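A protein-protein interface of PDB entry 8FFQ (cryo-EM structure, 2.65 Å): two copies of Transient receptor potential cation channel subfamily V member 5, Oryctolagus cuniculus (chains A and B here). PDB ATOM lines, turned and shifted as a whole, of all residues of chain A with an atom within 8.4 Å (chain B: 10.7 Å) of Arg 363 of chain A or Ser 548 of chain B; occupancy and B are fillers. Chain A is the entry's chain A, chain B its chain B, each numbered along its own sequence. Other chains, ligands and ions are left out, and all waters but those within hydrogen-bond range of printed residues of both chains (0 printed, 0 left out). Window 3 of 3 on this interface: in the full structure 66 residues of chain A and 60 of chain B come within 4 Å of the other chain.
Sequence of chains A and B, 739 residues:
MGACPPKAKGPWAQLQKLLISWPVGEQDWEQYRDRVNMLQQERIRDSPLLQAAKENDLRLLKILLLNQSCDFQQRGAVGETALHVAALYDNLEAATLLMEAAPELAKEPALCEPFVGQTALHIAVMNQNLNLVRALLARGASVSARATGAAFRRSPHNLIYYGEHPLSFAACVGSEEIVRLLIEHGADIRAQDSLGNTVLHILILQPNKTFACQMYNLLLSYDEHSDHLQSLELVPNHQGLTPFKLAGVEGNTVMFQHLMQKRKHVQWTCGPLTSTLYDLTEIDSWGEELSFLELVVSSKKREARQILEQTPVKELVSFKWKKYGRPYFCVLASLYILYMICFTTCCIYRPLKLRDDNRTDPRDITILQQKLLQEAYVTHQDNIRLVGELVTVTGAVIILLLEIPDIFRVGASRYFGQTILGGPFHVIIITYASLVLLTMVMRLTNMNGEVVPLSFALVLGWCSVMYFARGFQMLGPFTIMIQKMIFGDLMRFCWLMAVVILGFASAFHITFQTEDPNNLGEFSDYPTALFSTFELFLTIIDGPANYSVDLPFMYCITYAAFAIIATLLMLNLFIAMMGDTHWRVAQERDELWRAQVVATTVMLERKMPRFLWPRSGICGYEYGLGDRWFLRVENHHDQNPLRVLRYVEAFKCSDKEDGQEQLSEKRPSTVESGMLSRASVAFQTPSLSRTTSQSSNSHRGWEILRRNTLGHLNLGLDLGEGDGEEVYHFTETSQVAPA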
ATOM      1  N   ARG A 359     -37.798  15.765  15.384  1.00  0.00           N
ATOM      2  CA  ARG A 359     -37.029  14.505  15.333  1.00  0.00           C
ATOM      3  C   ARG A 359     -37.862  13.528  16.169  1.00  0.00           C
ATOM      4  O   ARG A 359     -38.389  13.963  17.205  1.00  0.00           O
ATOM      5  CB  ARG A 359     -35.566  14.679  15.774  1.00  0.00           C
ATOM      6  CG  ARG A 359     -34.828  15.830  15.119  1.00  0.00           C
ATOM      7  CD  ARG A 359     -34.073  16.581  16.193  1.00  0.00           C
ATOM      8  NE  ARG A 359     -32.809  15.973  16.567  1.00  0.00           N
ATOM      9  CZ  ARG A 359     -32.153  16.270  17.679  1.00  0.00           C
ATOM     10  NH1 ARG A 359     -30.996  15.690  17.946  1.00  0.00           N
ATOM     11  NH2 ARG A 359     -32.666  17.140  18.525  1.00  0.00           N
ATOM     12  N   THR A 360     -37.960  12.276  15.747  1.00  0.00           N
ATOM     13  CA  THR A 360     -38.773  11.214  16.356  1.00  0.00           C
ATOM     14  C   THR A 360     -37.899  10.144  17.006  1.00  0.00           C
ATOM     15  O   THR A 360     -37.812  10.076  18.229  1.00  0.00           O
ATOM     16  CB  THR A 360     -39.754  10.624  15.335  1.00  0.00           C
ATOM     17  OG1 THR A 360     -39.080  10.231  14.163  1.00  0.00           O
ATOM     18  CG2 THR A 360     -40.825  11.635  14.931  1.00  0.00           C
ATOM     19  N   ASP A 361     -37.213   9.318  16.226  1.00  0.00           N
ATOM     20  CA  ASP A 361     -36.308   8.283  16.716  1.00  0.00           C
ATOM     21  C   ASP A 361     -35.019   8.878  17.312  1.00  0.00           C
ATOM     22  O   ASP A 361     -34.478   9.847  16.774  1.00  0.00           O
ATOM     23  CB  ASP A 361     -35.989   7.253  15.621  1.00  0.00           C
ATOM     24  CG  ASP A 361     -35.441   7.793  14.293  1.00  0.00           C
ATOM     25  OD1 ASP A 361     -35.783   8.911  13.876  1.00  0.00           O
ATOM     26  OD2 ASP A 361     -34.713   7.038  13.626  1.00  0.00           O
ATOM     27  N   PRO A 362     -34.477   8.288  18.394  1.00  0.00           N
ATOM     28  CA  PRO A 362     -33.312   8.826  19.100  1.00  0.00           C
ATOM     29  C   PRO A 362     -32.051   8.852  18.226  1.00  0.00           C
ATOM     30  O   PRO A 362     -31.129   9.628  18.456  1.00  0.00           O
ATOM     31  CB  PRO A 362     -33.139   7.911  20.313  1.00  0.00           C
ATOM     32  CG  PRO A 362     -33.723   6.581  19.856  1.00  0.00           C
ATOM     33  CD  PRO A 362     -34.887   7.027  18.990  1.00  0.00           C
ATOM     34  N   ARG A 363     -32.111   8.087  17.129  1.00  0.00           N
ATOM     35  CA  ARG A 363     -30.934   7.927  16.235  1.00  0.00           C
ATOM     36  C   ARG A 363     -30.781   9.117  15.294  1.00  0.00           C
ATOM     37  O   ARG A 363     -29.690   9.242  14.745  1.00  0.00           O
ATOM     38  CB  ARG A 363     -31.102   6.592  15.516  1.00  0.00           C
ATOM     39  CG  ARG A 363     -30.079   6.258  14.451  1.00  0.00           C
ATOM     40  CD  ARG A 363     -30.314   4.797  14.127  1.00  0.00           C
ATOM     41  NE  ARG A 363     -29.554   3.994  15.065  1.00  0.00           N
ATOM     42  CZ  ARG A 363     -28.270   3.706  14.916  1.00  0.00           C
ATOM     43  NH1 ARG A 363     -27.647   2.977  15.823  1.00  0.00           N
ATOM     44  NH2 ARG A 363     -27.615   4.143  13.859  1.00  0.00           N
ATOM     45  N   ASP A 364     -31.825   9.936  15.112  1.00  0.00           N
ATOM     46  CA  ASP A 364     -31.739  11.169  14.317  1.00  0.00           C
ATOM     47  C   ASP A 364     -31.112  12.330  15.114  1.00  0.00           C
ATOM     48  O   ASP A 364     -31.637  12.752  16.145  1.00  0.00           O
ATOM     49  CB  ASP A 364     -33.133  11.535  13.769  1.00  0.00           C
ATOM     50  CG  ASP A 364     -33.154  12.746  12.820  1.00  0.00           C
ATOM     51  OD1 ASP A 364     -32.133  13.443  12.678  1.00  0.00           O
ATOM     52  OD2 ASP A 364     -34.201  13.017  12.189  1.00  0.00           O
ATOM     53  N   ILE A 365     -30.008  12.886  14.614  1.00  0.00           N
ATOM     54  CA  ILE A 365     -29.293  14.024  15.209  1.00  0.00           C
ATOM     55  C   ILE A 365     -29.326  15.292  14.353  1.00  0.00           C
ATOM     56  O   ILE A 365     -28.751  16.295  14.755  1.00  0.00           O
ATOM     57  CB  ILE A 365     -27.861  13.631  15.615  1.00  0.00           C
ATOM     58  CG1 ILE A 365     -26.982  13.245  14.409  1.00  0.00           C
ATOM     59  CG2 ILE A 365     -27.926  12.535  16.679  1.00  0.00           C
ATOM     60  CD1 ILE A 365     -25.488  13.220  14.710  1.00  0.00           C
ATOM     61  N   THR A 366     -30.009  15.314  13.213  1.00  0.00           N
ATOM     62  CA  THR A 366     -30.129  16.531  12.407  1.00  0.00           C
ATOM     63  C   THR A 366     -31.077  17.506  13.087  1.00  0.00           C
ATOM     64  O   THR A 366     -32.227  17.167  13.336  1.00  0.00           O
ATOM     65  CB  THR A 366     -30.615  16.212  10.995  1.00  0.00           C
ATOM     66  OG1 THR A 366     -29.664  15.436  10.315  1.00  0.00           O
ATOM     67  CG2 THR A 366     -30.849  17.453  10.147  1.00  0.00           C
ATOM     68  N   PRO A 517     -26.809  -5.309  18.900  1.00  0.00           N
ATOM     69  CA  PRO A 517     -26.002  -4.243  18.308  1.00  0.00           C
ATOM     70  C   PRO A 517     -25.732  -3.071  19.258  1.00  0.00           C
ATOM     71  O   PRO A 517     -24.716  -2.398  19.119  1.00  0.00           O
ATOM     72  CB  PRO A 517     -26.774  -3.794  17.067  1.00  0.00           C
ATOM     73  CG  PRO A 517     -28.216  -4.171  17.380  1.00  0.00           C
ATOM     74  CD  PRO A 517     -28.053  -5.463  18.166  1.00  0.00           C
ATOM     75  N   ASN A 518     -26.581  -2.834  20.259  1.00  0.00           N
ATOM     76  CA  ASN A 518     -26.356  -1.776  21.245  1.00  0.00           C
ATOM     77  C   ASN A 518     -25.187  -2.060  22.203  1.00  0.00           C
ATOM     78  O   ASN A 518     -24.654  -1.133  22.808  1.00  0.00           O
ATOM     79  CB  ASN A 518     -27.662  -1.508  22.004  1.00  0.00           C
ATOM     80  CG  ASN A 518     -28.759  -1.021  21.078  1.00  0.00           C
ATOM     81  OD1 ASN A 518     -29.676  -1.742  20.721  1.00  0.00           O
ATOM     82  ND2 ASN A 518     -28.683   0.204  20.624  1.00  0.00           N
ATOM     83  N   ASN A 519     -24.749  -3.312  22.333  1.00  0.00           N
ATOM     84  CA  ASN A 519     -23.596  -3.674  23.152  1.00  0.00           C
ATOM     85  C   ASN A 519     -22.254  -3.649  22.400  1.00  0.00           C
ATOM     86  O   ASN A 519     -21.224  -3.482  23.045  1.00  0.00           O
ATOM     87  CB  ASN A 519     -23.885  -5.022  23.825  1.00  0.00           C
ATOM     88  CG  ASN A 519     -24.655  -4.815  25.115  1.00  0.00           C
ATOM     89  OD1 ASN A 519     -24.099  -4.428  26.125  1.00  0.00           O
ATOM     90  ND2 ASN A 519     -25.940  -5.020  25.152  1.00  0.00           N
ATOM     91  N   GLY A 521     -21.366  -1.854  18.507  1.00  0.00           N
ATOM     92  CA  GLY A 521     -22.010  -1.265  17.332  1.00  0.00           C
ATOM     93  C   GLY A 521     -21.215  -1.348  16.036  1.00  0.00           C
ATOM     94  O   GLY A 521     -21.801  -1.244  14.959  1.00  0.00           O
ATOM     95  N   GLU A 522     -19.905  -1.561  16.112  1.00  0.00           N
ATOM     96  CA  GLU A 522     -18.967  -1.484  14.991  1.00  0.00           C
ATOM     97  C   GLU A 522     -19.335  -2.385  13.820  1.00  0.00           C
ATOM     98  O   GLU A 522     -19.121  -2.026  12.669  1.00  0.00           O
ATOM     99  CB  GLU A 522     -17.557  -1.862  15.475  1.00  0.00           C
ATOM    100  CG  GLU A 522     -16.887  -0.770  16.312  1.00  0.00           C
ATOM    101  CD  GLU A 522     -17.221  -0.746  17.821  1.00  0.00           C
ATOM    102  OE1 GLU A 522     -18.175  -1.414  18.266  1.00  0.00           O
ATOM    103  OE2 GLU A 522     -16.535  -0.008  18.559  1.00  0.00           O
ATOM    104  N   SER A 524     -22.576  -3.797  13.357  1.00  0.00           N
ATOM    105  CA  SER A 524     -24.039  -3.919  13.492  1.00  0.00           C
ATOM    106  C   SER A 524     -24.794  -4.141  12.172  1.00  0.00           C
ATOM    107  O   SER A 524     -25.800  -4.844  12.151  1.00  0.00           O
ATOM    108  CB  SER A 524     -24.598  -2.689  14.213  1.00  0.00           C
ATOM    109  OG  SER A 524     -24.148  -1.485  13.624  1.00  0.00           O
ATOM    110  N   ASP A 525     -24.297  -3.605  11.064  1.00  0.00           N
ATOM    111  CA  ASP A 525     -24.759  -3.879   9.701  1.00  0.00           C
ATOM    112  C   ASP A 525     -23.560  -3.925   8.751  1.00  0.00           C
ATOM    113  O   ASP A 525     -22.468  -3.486   9.105  1.00  0.00           O
ATOM    114  CB  ASP A 525     -25.822  -2.864   9.258  1.00  0.00           C
ATOM    115  CG  ASP A 525     -25.360  -1.408   9.313  1.00  0.00           C
ATOM    116  OD1 ASP A 525     -24.279  -1.087   8.775  1.00  0.00           O
ATOM    117  OD2 ASP A 525     -26.094  -0.574   9.878  1.00  0.00           O
ATOM    118  N   THR A 528     -21.542  -0.648   7.945  1.00  0.00           N
ATOM    119  CA  THR A 528     -20.799  -0.239   9.137  1.00  0.00           C
ATOM    120  C   THR A 528     -19.658  -1.203   9.416  1.00  0.00           C
ATOM    121  O   THR A 528     -18.578  -0.766   9.781  1.00  0.00           O
ATOM    122  CB  THR A 528     -21.709  -0.162  10.364  1.00  0.00           C
ATOM    123  OG1 THR A 528     -22.839   0.601  10.053  1.00  0.00           O
ATOM    124  CG2 THR A 528     -21.044   0.539  11.541  1.00  0.00           C
ATOM    125  N   PHE B 512     -20.983  18.534   9.649  1.00  0.00           N
ATOM    126  CA  PHE B 512     -21.602  18.476  10.972  1.00  0.00           C
ATOM    127  C   PHE B 512     -22.430  19.699  11.365  1.00  0.00           C
ATOM    128  O   PHE B 512     -23.179  19.610  12.327  1.00  0.00           O
ATOM    129  CB  PHE B 512     -20.549  18.111  12.023  1.00  0.00           C
ATOM    130  CG  PHE B 512     -20.353  16.618  12.043  1.00  0.00           C
ATOM    131  CD1 PHE B 512     -21.243  15.809  12.766  1.00  0.00           C
ATOM    132  CD2 PHE B 512     -19.370  16.024  11.243  1.00  0.00           C
ATOM    133  CE1 PHE B 512     -21.159  14.413  12.681  1.00  0.00           C
ATOM    134  CE2 PHE B 512     -19.277  14.633  11.171  1.00  0.00           C
ATOM    135  CZ  PHE B 512     -20.174  13.824  11.881  1.00  0.00           C
ATOM    136  N   GLU B 515     -26.047  19.002  12.182  1.00  0.00           N
ATOM    137  CA  GLU B 515     -26.219  18.017  13.240  1.00  0.00           C
ATOM    138  C   GLU B 515     -26.055  18.612  14.641  1.00  0.00           C
ATOM    139  O   GLU B 515     -25.435  19.652  14.848  1.00  0.00           O
ATOM    140  CB  GLU B 515     -25.214  16.868  13.060  1.00  0.00           C
ATOM    141  CG  GLU B 515     -25.026  16.324  11.634  1.00  0.00           C
ATOM    142  CD  GLU B 515     -26.332  15.999  10.894  1.00  0.00           C
ATOM    143  OE1 GLU B 515     -27.332  15.639  11.535  1.00  0.00           O
ATOM    144  OE2 GLU B 515     -26.355  16.091   9.654  1.00  0.00           O
ATOM    145  N   ASP B 516     -26.582  17.914  15.632  1.00  0.00           N
ATOM    146  CA  ASP B 516     -26.507  18.272  17.039  1.00  0.00           C
ATOM    147  C   ASP B 516     -25.078  18.124  17.602  1.00  0.00           C
ATOM    148  O   ASP B 516     -24.574  17.001  17.683  1.00  0.00           O
ATOM    149  CB  ASP B 516     -27.491  17.369  17.781  1.00  0.00           C
ATOM    150  CG  ASP B 516     -27.463  17.582  19.284  1.00  0.00           C
ATOM    151  OD1 ASP B 516     -27.145  18.692  19.740  1.00  0.00           O
ATOM    152  OD2 ASP B 516     -27.756  16.616  19.997  1.00  0.00           O
ATOM    153  N   ASN B 518     -23.813  18.050  20.562  1.00  0.00           N
ATOM    154  CA  ASN B 518     -23.703  17.167  21.725  1.00  0.00           C
ATOM    155  C   ASN B 518     -23.606  15.676  21.362  1.00  0.00           C
ATOM    156  O   ASN B 518     -23.141  14.879  22.174  1.00  0.00           O
ATOM    157  CB  ASN B 518     -24.869  17.445  22.682  1.00  0.00           C
ATOM    158  CG  ASN B 518     -24.836  18.868  23.205  1.00  0.00           C
ATOM    159  OD1 ASN B 518     -25.596  19.729  22.794  1.00  0.00           O
ATOM    160  ND2 ASN B 518     -23.931  19.175  24.098  1.00  0.00           N
ATOM    161  N   ASN B 519     -24.001  15.278  20.152  1.00  0.00           N
ATOM    162  CA  ASN B 519     -23.873  13.901  19.682  1.00  0.00           C
ATOM    163  C   ASN B 519     -22.545  13.596  18.970  1.00  0.00           C
ATOM    164  O   ASN B 519     -22.143  12.437  18.951  1.00  0.00           O
ATOM    165  CB  ASN B 519     -25.105  13.567  18.832  1.00  0.00           C
ATOM    166  CG  ASN B 519     -26.245  13.092  19.713  1.00  0.00           C
ATOM    167  OD1 ASN B 519     -26.257  11.968  20.177  1.00  0.00           O
ATOM    168  ND2 ASN B 519     -27.220  13.900  20.015  1.00  0.00           N
ATOM    169  N   LEU B 520     -21.834  14.589  18.430  1.00  0.00           N
ATOM    170  CA  LEU B 520     -20.465  14.435  17.930  1.00  0.00           C
ATOM    171  C   LEU B 520     -19.764  15.801  17.976  1.00  0.00           C
ATOM    172  O   LEU B 520     -20.057  16.698  17.190  1.00  0.00           O
ATOM    173  CB  LEU B 520     -20.494  13.782  16.529  1.00  0.00           C
ATOM    174  CG  LEU B 520     -19.117  13.267  16.068  1.00  0.00           C
ATOM    175  CD1 LEU B 520     -19.278  12.055  15.157  1.00  0.00           C
ATOM    176  CD2 LEU B 520     -18.326  14.331  15.315  1.00  0.00           C
ATOM    177  N   PRO B 544     -13.840   9.922  14.908  1.00  0.00           N
ATOM    178  CA  PRO B 544     -15.119  10.227  15.522  1.00  0.00           C
ATOM    179  C   PRO B 544     -16.155   9.165  15.182  1.00  0.00           C
ATOM    180  O   PRO B 544     -16.328   8.805  14.022  1.00  0.00           O
ATOM    181  CB  PRO B 544     -15.505  11.619  15.027  1.00  0.00           C
ATOM    182  CG  PRO B 544     -14.147  12.244  14.771  1.00  0.00           C
ATOM    183  CD  PRO B 544     -13.332  11.092  14.222  1.00  0.00           C
ATOM    184  N   ALA B 545     -16.817   8.642  16.197  1.00  0.00           N
ATOM    185  CA  ALA B 545     -17.819   7.605  16.065  1.00  0.00           C
ATOM    186  C   ALA B 545     -18.869   7.749  17.161  1.00  0.00           C
ATOM    187  O   ALA B 545     -18.554   8.014  18.323  1.00  0.00           O
ATOM    188  CB  ALA B 545     -17.141   6.233  16.122  1.00  0.00           C
ATOM    189  N   ASN B 546     -20.117   7.507  16.791  1.00  0.00           N
ATOM    190  CA  ASN B 546     -21.206   7.331  17.728  1.00  0.00           C
ATOM    191  C   ASN B 546     -22.188   6.345  17.092  1.00  0.00           C
ATOM    192  O   ASN B 546     -23.072   6.709  16.346  1.00  0.00           O
ATOM    193  CB  ASN B 546     -21.768   8.710  18.071  1.00  0.00           C
ATOM    194  CG  ASN B 546     -22.850   8.748  19.109  1.00  0.00           C
ATOM    195  OD1 ASN B 546     -23.349   7.728  19.547  1.00  0.00           O
ATOM    196  ND2 ASN B 546     -23.253   9.896  19.570  1.00  0.00           N
ATOM    197  N   TYR B 547     -22.024   5.053  17.382  1.00  0.00           N
ATOM    198  CA  TYR B 547     -22.848   4.004  16.801  1.00  0.00           C
ATOM    199  C   TYR B 547     -24.322   4.034  17.216  1.00  0.00           C
ATOM    200  O   TYR B 547     -25.167   3.408  16.591  1.00  0.00           O
ATOM    201  CB  TYR B 547     -22.179   2.626  16.990  1.00  0.00           C
ATOM    202  CG  TYR B 547     -20.834   2.541  16.284  1.00  0.00           C
ATOM    203  CD1 TYR B 547     -20.773   2.481  14.875  1.00  0.00           C
ATOM    204  CD2 TYR B 547     -19.632   2.518  17.019  1.00  0.00           C
ATOM    205  CE1 TYR B 547     -19.526   2.414  14.221  1.00  0.00           C
ATOM    206  CE2 TYR B 547     -18.389   2.453  16.386  1.00  0.00           C
ATOM    207  CZ  TYR B 547     -18.326   2.412  14.966  1.00  0.00           C
ATOM    208  OH  TYR B 547     -17.137   2.311  14.316  1.00  0.00           O
ATOM    209  N   SER B 548     -24.670   4.775  18.272  1.00  0.00           N
ATOM    210  CA  SER B 548     -26.055   4.993  18.764  1.00  0.00           C
ATOM    211  C   SER B 548     -26.858   5.986  17.896  1.00  0.00           C
ATOM    212  O   SER B 548     -28.031   6.149  18.137  1.00  0.00           O
ATOM    213  CB  SER B 548     -26.076   5.532  20.190  1.00  0.00           C
ATOM    214  OG  SER B 548     -25.302   4.728  21.074  1.00  0.00           O
ATOM    215  N   VAL B 549     -26.248   6.674  16.907  1.00  0.00           N
ATOM    216  CA  VAL B 549     -26.888   7.701  16.112  1.00  0.00           C
ATOM    217  C   VAL B 549     -26.546   7.590  14.611  1.00  0.00           C
ATOM    218  O   VAL B 549     -25.493   7.036  14.265  1.00  0.00           O
ATOM    219  CB  VAL B 549     -26.579   9.133  16.617  1.00  0.00           C
ATOM    220  CG1 VAL B 549     -27.004   9.365  18.046  1.00  0.00           C
ATOM    221  CG2 VAL B 549     -25.106   9.500  16.493  1.00  0.00           C
ATOM    222  N   ASP B 550     -27.356   8.152  13.739  1.00  0.00           N
ATOM    223  CA  ASP B 550     -27.109   8.169  12.289  1.00  0.00           C
ATOM    224  C   ASP B 550     -26.273   9.413  11.904  1.00  0.00           C
ATOM    225  O   ASP B 550     -26.799  10.521  11.686  1.00  0.00           O
ATOM    226  CB  ASP B 550     -28.420   8.060  11.523  1.00  0.00           C
ATOM    227  CG  ASP B 550     -29.037   6.645  11.587  1.00  0.00           C
ATOM    228  OD1 ASP B 550     -28.440   5.717  12.197  1.00  0.00           O
ATOM    229  OD2 ASP B 550     -30.053   6.407  10.908  1.00  0.00           O
ATOM    230  N   LEU B 551     -24.962   9.219  11.753  1.00  0.00           N
ATOM    231  CA  LEU B 551     -24.047  10.221  11.195  1.00  0.00           C
ATOM    232  C   LEU B 551     -24.350  10.508   9.708  1.00  0.00           C
ATOM    233  O   LEU B 551     -24.796   9.608   8.992  1.00  0.00           O
ATOM    234  CB  LEU B 551     -22.587   9.764  11.372  1.00  0.00           C
ATOM    235  CG  LEU B 551     -22.164   9.418  12.807  1.00  0.00           C
ATOM    236  CD1 LEU B 551     -20.675   9.123  12.859  1.00  0.00           C
ATOM    237  CD2 LEU B 551     -22.433  10.565  13.766  1.00  0.00           C
ATOM    238  N   PRO B 552     -24.107  11.731   9.205  1.00  0.00           N
ATOM    239  CA  PRO B 552     -24.322  12.064   7.800  1.00  0.00           C
ATOM    240  C   PRO B 552     -23.410  11.248   6.870  1.00  0.00           C
ATOM    241  O   PRO B 552     -22.211  11.150   7.100  1.00  0.00           O
ATOM    242  CB  PRO B 552     -24.060  13.570   7.707  1.00  0.00           C
ATOM    243  CG  PRO B 552     -23.127  13.859   8.876  1.00  0.00           C
ATOM    244  CD  PRO B 552     -23.599  12.880   9.934  1.00  0.00           C
ATOM    245  N   CYS B 556     -18.702   9.664   6.461  1.00  0.00           N
ATOM    246  CA  CYS B 556     -18.059   8.381   6.205  1.00  0.00           C
ATOM    247  C   CYS B 556     -17.178   8.497   4.955  1.00  0.00           C
ATOM    248  O   CYS B 556     -16.003   8.130   5.022  1.00  0.00           O
ATOM    249  CB  CYS B 556     -19.135   7.288   6.112  1.00  0.00           C
ATOM    250  SG  CYS B 556     -19.960   7.144   7.696  1.00  0.00           S
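Printed residues of chain A within 4 Å of Ser 548 of chain B: Arg 363. No residue of chain B comes within 4 Å of Asp 364 of chain A. Val 549 of chain B touches just these residues of chain A: Arg 363 (3.5 Å) and Ile 365 (3.6 Å). Of the printed residues of chain B, Arg 359 of chain A touches Asp 516. Printed residues of chain A within 4 Å of Asp 516 of chain B: Arg 359 (3.9 Å) and Ile 365 (2.8 Å). Of the printed residues of chain A, Glu 515 of chain B touches Ile 365 (3.4 Å) and Thr 366 (2.6 Å). The nearest residue of chain B that does not touch Arg 363 of chain A is Leu 551 of chain B (5.6 Å). The nearest residue of chain A that does not touch Ser 548 of chain B is Pro 362 of chain A (4.7 Å).
Positions printed for both chains: 518 and 519. Of the 14 pairs that touch across the chains among the printed residues, none has its exchanged pair printed and touching as well.
The guanidinium group of Arg 363 of chain A is in hydrogen-bond range of the backbone carbonyl oxygen of Tyr 547 of chain B (2.6 Å). The backbone carbonyl oxygen of Ile 365 of chain A sits at hydrogen-bond distance from the backbone NH of Asp 516 of chain B (2.8 Å). The guanidinium group of Arg 363 of chain A lies within salt-bridge range of the side-chain carboxylate of Asp 550 of chain B (2.4 Å). The guanidinium group (NH1) of Arg 359 of chain A lies within salt-bridge range of the side-chain carboxylate (OD2) of Asp 516 of chain B (3.9 Å). The side-chain carboxylate of Glu 515 of chain B sits at hydrogen-bond distance from the side-chain hydroxyl of Thr 366 of chain A, at 2.6 Å.
OD1 of Asn 546 of chain B sits close to N of Ser 548 of chain B. The backbone NH of Asn 518 of chain B sits close to the side-chain carboxylate of Asp 516 of chain B, 3.5 Å away. The backbone carbonyl oxygen (O) of Asn 519 of chain B is in hydrogen-bond range of the side-chain amide nitrogen (ND2) of Asn 546 of chain B, at 2.8 Å. The backbone carbonyl oxygen (O) of Thr 366 of chain A lies close to the guanidinium group (NE) of Arg 359 of chain A, at 3.5 Å. The backbone carbonyl oxygen (O) of Gly 521 of chain A sits at hydrogen-bond distance from the side-chain hydroxyl (OG) of Ser 524 of chain A, 2.7 Å away. OD1 of Asp 525 of chain A is in hydrogen-bond range of OG1 of Thr 528 of chain A (2.6 Å).
Among the printed residues, merely in contact across the chains: Ile 365 of chain A with Glu 515 of chain B (3.4 Å), Arg 363 of chain A with Val 549 of chain B (3.5 Å), Ile 365 of chain A with Asn 519 of chain B (3.5 Å), Glu 522 of chain A with Tyr 547 of chain B (3.6 Å), Ile 365 of chain A with Val 549 of chain B (3.6 Å), Thr 528 of chain A with Tyr 547 of chain B (3.6 Å), Arg 363 of chain A with Ser 548 of chain B (3.7 Å), Ile 365 of chain A with Asp 550 of chain B (3.9 Å) and Gly 521 of chain A with Tyr 547 of chain B (3.9 Å).
Printed residues of chain A that touch a printed residue of chain B: Arg 359, Arg 363, Ile 365, Thr 366, Gly 521, Glu 522 and Thr 528. Hydrophobic or aromatic side chains of chain A within 4 Å of the printed part of chain B: Ile 365. Hydrophobic or aromatic side chains of chain B within 4 Å of the printed part of chain A: Tyr 547 and Val 549. Among the printed residues, 14 pairs touch across the chains.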
